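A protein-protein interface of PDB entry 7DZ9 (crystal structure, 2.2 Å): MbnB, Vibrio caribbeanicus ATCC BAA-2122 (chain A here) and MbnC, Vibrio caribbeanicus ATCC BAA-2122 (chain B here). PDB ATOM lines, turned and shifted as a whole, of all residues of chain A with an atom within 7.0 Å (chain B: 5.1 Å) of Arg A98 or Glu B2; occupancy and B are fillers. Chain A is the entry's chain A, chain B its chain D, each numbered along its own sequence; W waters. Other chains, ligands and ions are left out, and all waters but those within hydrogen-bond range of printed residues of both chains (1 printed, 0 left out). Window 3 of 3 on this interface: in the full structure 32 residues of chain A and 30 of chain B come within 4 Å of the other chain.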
ATOM      1  N   LYS A  94     -14.332   2.162   0.106  1.00  0.00           N
ATOM      2  CA  LYS A  94     -15.034   1.009   0.648  1.00  0.00           C
ATOM      3  C   LYS A  94     -14.012  -0.035   1.082  1.00  0.00           C
ATOM      4  O   LYS A  94     -13.165  -0.449   0.281  1.00  0.00           O
ATOM      5  CB  LYS A  94     -15.994   0.436  -0.396  1.00  0.00           C
ATOM      6  CG  LYS A  94     -16.627  -0.875  -0.013  1.00  0.00           C
ATOM      7  CD  LYS A  94     -17.248  -1.497  -1.230  1.00  0.00           C
ATOM      8  CE  LYS A  94     -18.735  -1.677  -1.042  1.00  0.00           C
ATOM      9  NZ  LYS A  94     -19.437  -0.381  -1.057  1.00  0.00           N
ATOM     10  N   TYR A  96     -14.968  -2.902   3.349  1.00  0.00           N
ATOM     11  CA  TYR A  96     -15.634  -4.125   3.749  1.00  0.00           C
ATOM     12  C   TYR A  96     -16.728  -4.411   2.738  1.00  0.00           C
ATOM     13  O   TYR A  96     -17.275  -3.489   2.120  1.00  0.00           O
ATOM     14  CB  TYR A  96     -16.266  -4.014   5.151  1.00  0.00           C
ATOM     15  CG  TYR A  96     -15.266  -3.654   6.205  1.00  0.00           C
ATOM     16  CD1 TYR A  96     -14.969  -2.323   6.465  1.00  0.00           C
ATOM     17  CD2 TYR A  96     -14.575  -4.644   6.911  1.00  0.00           C
ATOM     18  CE1 TYR A  96     -14.040  -1.977   7.415  1.00  0.00           C
ATOM     19  CE2 TYR A  96     -13.624  -4.304   7.867  1.00  0.00           C
ATOM     20  CZ  TYR A  96     -13.365  -2.967   8.108  1.00  0.00           C
ATOM     21  OH  TYR A  96     -12.429  -2.600   9.043  1.00  0.00           O
ATOM     22  N   HIS A  97     -17.059  -5.695   2.606  1.00  0.00           N
ATOM     23  CA  HIS A  97     -18.210  -6.128   1.829  1.00  0.00           C
ATOM     24  C   HIS A  97     -18.824  -7.296   2.586  1.00  0.00           C
ATOM     25  O   HIS A  97     -18.136  -8.289   2.843  1.00  0.00           O
ATOM     26  CB  HIS A  97     -17.801  -6.555   0.424  1.00  0.00           C
ATOM     27  CG  HIS A  97     -18.936  -7.026  -0.428  1.00  0.00           C
ATOM     28  ND1 HIS A  97     -20.074  -6.279  -0.621  1.00  0.00           N
ATOM     29  CD2 HIS A  97     -19.118  -8.178  -1.116  1.00  0.00           C
ATOM     30  CE1 HIS A  97     -20.906  -6.942  -1.401  1.00  0.00           C
ATOM     31  NE2 HIS A  97     -20.350  -8.099  -1.714  1.00  0.00           N
ATOM     32  N   ARG A  98     -20.091  -7.166   2.995  1.00  0.00           N
ATOM     33  CA  ARG A  98     -20.739  -8.212   3.791  1.00  0.00           C
ATOM     34  C   ARG A  98     -19.956  -8.570   5.042  1.00  0.00           C
ATOM     35  O   ARG A  98     -19.934  -9.731   5.440  1.00  0.00           O
ATOM     36  CB  ARG A  98     -20.949  -9.505   2.993  1.00  0.00           C
ATOM     37  CG  ARG A  98     -21.437  -9.392   1.582  1.00  0.00           C
ATOM     38  CD  ARG A  98     -22.811  -9.886   1.557  1.00  0.00           C
ATOM     39  NE  ARG A  98     -23.365 -10.111   0.226  1.00  0.00           N
ATOM     40  CZ  ARG A  98     -24.622 -10.511   0.021  1.00  0.00           C
ATOM     41  NH1 ARG A  98     -25.440 -10.799   1.039  1.00  0.00           N
ATOM     42  NH2 ARG A  98     -25.031 -10.715  -1.237  1.00  0.00           N
ATOM     43  N   GLY A  99     -19.277  -7.595   5.648  1.00  0.00           N
ATOM     44  CA  GLY A  99     -18.517  -7.871   6.855  1.00  0.00           C
ATOM     45  C   GLY A  99     -17.125  -8.440   6.646  1.00  0.00           C
ATOM     46  O   GLY A  99     -16.400  -8.648   7.632  1.00  0.00           O
ATOM     47  N   GLN A 100     -16.744  -8.767   5.415  1.00  0.00           N
ATOM     48  CA  GLN A 100     -15.392  -9.253   5.148  1.00  0.00           C
ATOM     49  C   GLN A 100     -14.508  -8.067   4.772  1.00  0.00           C
ATOM     50  O   GLN A 100     -14.900  -7.226   3.957  1.00  0.00           O
ATOM     51  CB  GLN A 100     -15.386 -10.297   4.034  1.00  0.00           C
ATOM     52  CG  GLN A 100     -16.143 -11.587   4.348  1.00  0.00           C
ATOM     53  CD  GLN A 100     -15.513 -12.386   5.470  1.00  0.00           C
ATOM     54  OE1 GLN A 100     -16.000 -12.387   6.591  1.00  0.00           O
ATOM     55  NE2 GLN A 100     -14.419 -13.062   5.174  1.00  0.00           N
ATOM     56  N   ALA A 101     -13.334  -7.985   5.390  1.00  0.00           N
ATOM     57  CA  ALA A 101     -12.389  -6.925   5.060  1.00  0.00           C
ATOM     58  C   ALA A 101     -11.798  -7.136   3.668  1.00  0.00           C
ATOM     59  O   ALA A 101     -11.327  -8.231   3.342  1.00  0.00           O
ATOM     60  CB  ALA A 101     -11.261  -6.870   6.097  1.00  0.00           C
ATOM     61  N   LEU A 112     -26.054   4.855  -3.998  1.00  0.00           N
ATOM     62  CA  LEU A 112     -26.741   4.010  -3.032  1.00  0.00           C
ATOM     63  C   LEU A 112     -26.744   4.706  -1.674  1.00  0.00           C
ATOM     64  O   LEU A 112     -25.689   4.883  -1.056  1.00  0.00           O
ATOM     65  CB  LEU A 112     -26.066   2.645  -2.965  1.00  0.00           C
ATOM     66  CG  LEU A 112     -26.651   1.643  -1.979  1.00  0.00           C
ATOM     67  CD1 LEU A 112     -28.051   1.187  -2.419  1.00  0.00           C
ATOM     68  CD2 LEU A 112     -25.702   0.464  -1.853  1.00  0.00           C
ATOM     69  N   MET B   1     -20.206  -3.294  -9.303  1.00  0.00           N
ATOM     70  CA  MET B   1     -21.388  -4.122  -9.069  1.00  0.00           C
ATOM     71  C   MET B   1     -21.228  -4.929  -7.786  1.00  0.00           C
ATOM     72  O   MET B   1     -20.124  -5.110  -7.259  1.00  0.00           O
ATOM     73  CB  MET B   1     -21.603  -5.078 -10.257  1.00  0.00           C
ATOM     74  CG  MET B   1     -22.630  -4.616 -11.276  1.00  0.00           C
ATOM     75  SD  MET B   1     -24.242  -4.261 -10.528  1.00  0.00           S
ATOM     76  CE  MET B   1     -24.760  -2.876 -11.542  1.00  0.00           C
ATOM     77  N   GLU B   2     -22.356  -5.469  -7.279  1.00  0.00           N
ATOM     78  CA  GLU B   2     -22.209  -6.310  -6.100  1.00  0.00           C
ATOM     79  C   GLU B   2     -21.755  -7.692  -6.506  1.00  0.00           C
ATOM     80  O   GLU B   2     -21.246  -8.437  -5.677  1.00  0.00           O
ATOM     81  CB  GLU B   2     -23.508  -6.365  -5.281  1.00  0.00           C
ATOM     82  CG  GLU B   2     -23.302  -7.127  -3.969  1.00  0.00           C
ATOM     83  CD  GLU B   2     -24.142  -6.630  -2.807  1.00  0.00           C
ATOM     84  OE1 GLU B   2     -24.926  -7.445  -2.273  1.00  0.00           O
ATOM     85  OE2 GLU B   2     -24.010  -5.442  -2.420  1.00  0.00           O
ATOM     86  N   GLU B   3     -21.888  -8.030  -7.783  1.00  0.00           N
ATOM     87  CA  GLU B   3     -21.355  -9.303  -8.257  1.00  0.00           C
ATOM     88  C   GLU B   3     -19.830  -9.296  -8.244  1.00  0.00           C
ATOM     89  O   GLU B   3     -19.196 -10.298  -7.895  1.00  0.00           O
ATOM     90  CB  GLU B   3     -21.883  -9.592  -9.668  1.00  0.00           C
ATOM     91  CG  GLU B   3     -21.448 -10.933 -10.219  1.00  0.00           C
ATOM     92  CD  GLU B   3     -22.612 -11.755 -10.743  1.00  0.00           C
ATOM     93  OE1 GLU B   3     -23.698 -11.690 -10.125  1.00  0.00           O
ATOM     94  OE2 GLU B   3     -22.444 -12.469 -11.762  1.00  0.00           O
ATOM     95  N   ILE B   4     -19.228  -8.173  -8.614  1.00  0.00           N
ATOM     96  CA  ILE B   4     -17.775  -8.060  -8.543  1.00  0.00           C
ATOM     97  C   ILE B   4     -17.321  -8.135  -7.093  1.00  0.00           C
ATOM     98  O   ILE B   4     -16.356  -8.830  -6.765  1.00  0.00           O
ATOM     99  CB  ILE B   4     -17.318  -6.760  -9.223  1.00  0.00           C
ATOM    100  CG1 ILE B   4     -17.459  -6.905 -10.734  1.00  0.00           C
ATOM    101  CG2 ILE B   4     -15.896  -6.414  -8.841  1.00  0.00           C
ATOM    102  CD1 ILE B   4     -17.847  -5.624 -11.423  1.00  0.00           C
ATOM    103  N   LEU B   5     -18.020  -7.432  -6.202  1.00  0.00           N
ATOM    104  CA  LEU B   5     -17.701  -7.501  -4.780  1.00  0.00           C
ATOM    105  C   LEU B   5     -17.887  -8.913  -4.242  1.00  0.00           C
ATOM    106  O   LEU B   5     -17.020  -9.444  -3.542  1.00  0.00           O
ATOM    107  CB  LEU B   5     -18.571  -6.510  -4.020  1.00  0.00           C
ATOM    108  CG  LEU B   5     -18.302  -5.054  -4.383  1.00  0.00           C
ATOM    109  CD1 LEU B   5     -19.360  -4.134  -3.774  1.00  0.00           C
ATOM    110  CD2 LEU B   5     -16.929  -4.701  -3.878  1.00  0.00           C
ATOM    111  N   ASP B   6     -19.003  -9.559  -4.594  1.00  0.00           N
ATOM    112  CA  ASP B   6     -19.244 -10.925  -4.137  1.00  0.00           C
ATOM    113  C   ASP B   6     -18.105 -11.858  -4.539  1.00  0.00           C
ATOM    114  O   ASP B   6     -17.681 -12.702  -3.742  1.00  0.00           O
ATOM    115  CB  ASP B   6     -20.563 -11.446  -4.705  1.00  0.00           C
ATOM    116  CG  ASP B   6     -21.766 -10.921  -3.968  1.00  0.00           C
ATOM    117  OD1 ASP B   6     -21.593 -10.321  -2.887  1.00  0.00           O
ATOM    118  OD2 ASP B   6     -22.890 -11.108  -4.476  1.00  0.00           O
ATOM    119  N   ARG B   7     -17.584 -11.719  -5.768  1.00  0.00           N
ATOM    120  CA  ARG B   7     -16.534 -12.631  -6.210  1.00  0.00           C
ATOM    121  C   ARG B   7     -15.205 -12.318  -5.550  1.00  0.00           C
ATOM    122  O   ARG B   7     -14.337 -13.195  -5.478  1.00  0.00           O
ATOM    123  CB  ARG B   7     -16.347 -12.589  -7.737  1.00  0.00           C
ATOM    124  CG  ARG B   7     -17.604 -12.929  -8.524  1.00  0.00           C
ATOM    125  CD  ARG B   7     -17.795 -14.456  -8.664  1.00  0.00           C
ATOM    126  NE  ARG B   7     -18.270 -15.138  -7.443  1.00  0.00           N
ATOM    127  CZ  ARG B   7     -19.249 -14.722  -6.628  1.00  0.00           C
ATOM    128  NH1 ARG B   7     -19.912 -13.592  -6.865  1.00  0.00           N
ATOM    129  NH2 ARG B   7     -19.571 -15.442  -5.556  1.00  0.00           N
ATOM    130  N   ILE B   9     -14.930 -11.579  -2.239  1.00  0.00           N
ATOM    131  CA  ILE B   9     -14.954 -12.251  -0.942  1.00  0.00           C
ATOM    132  C   ILE B   9     -15.338 -13.717  -1.065  1.00  0.00           C
ATOM    133  O   ILE B   9     -15.044 -14.508  -0.154  1.00  0.00           O
ATOM    134  CB  ILE B   9     -15.917 -11.580   0.062  1.00  0.00           C
ATOM    135  CG1 ILE B   9     -17.371 -11.665  -0.421  1.00  0.00           C
ATOM    136  CG2 ILE B   9     -15.487 -10.139   0.365  1.00  0.00           C
ATOM    137  CD1 ILE B   9     -18.411 -11.246   0.646  1.00  0.00           C
HETATM  138  O   HOH W   1     -13.543 -13.906   2.390  1.00  0.00           O
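OD1 of Asp B6 lies within salt-bridge range of NE of Arg A98. NH2 of Arg A98 is in salt-bridge range of OE1 of Glu B2, at 3.4 Å. NE2 of His A97 lies within hydrogen-bond range of OD1 of Asp B6, at 2.8 Å.
Of chain B, only Glu B2 (3.4 Å), Asp B6 (3.6 Å) and Ile B9 (3.7 Å) come within 4 Å of Arg A98. Glu B2 touches just these residues of chain A: His A97 (3.5 Å) and Arg A98 (3.4 Å). Of the printed residues of chain B, Gln A100 touches Ile B9. Of the printed residues of chain A, Leu B5 touches Lys A94 and His A97. Of the printed residues of chain A, Ile B9 touches His A97 (3.6 Å), Arg A98 (3.7 Å) and Gln A100 (3.7 Å). Of the printed residues of chain B, Lys A94 touches Leu B5 (3.7 Å).
Of the 8 printed residues of chain A, 4 touch a printed residue of chain B. Among the printed residues, Asp or Glu carboxylates within 4 Å of a Lys or Arg side-chain nitrogen of the other chain: Arg A98 with Glu B2 and Arg A98 with Asp B6.
Water W1 bridges the backbone carbonyl oxygen of Ile B9 (3.0 Å) and the side-chain amide nitrogen of Gln A100 (3.0 Å).
Among the printed residues, merely in contact across the chains: Lys A94 with Leu B5 (3.7 Å), His A97 with Glu B2 (3.5 Å), His A97 with Leu B5 (3.3 Å), His A97 with Ile B9 (3.6 Å), Arg A98 with Ile B9 (3.7 Å) and Gln A100 with Ile B9 (3.7 Å).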
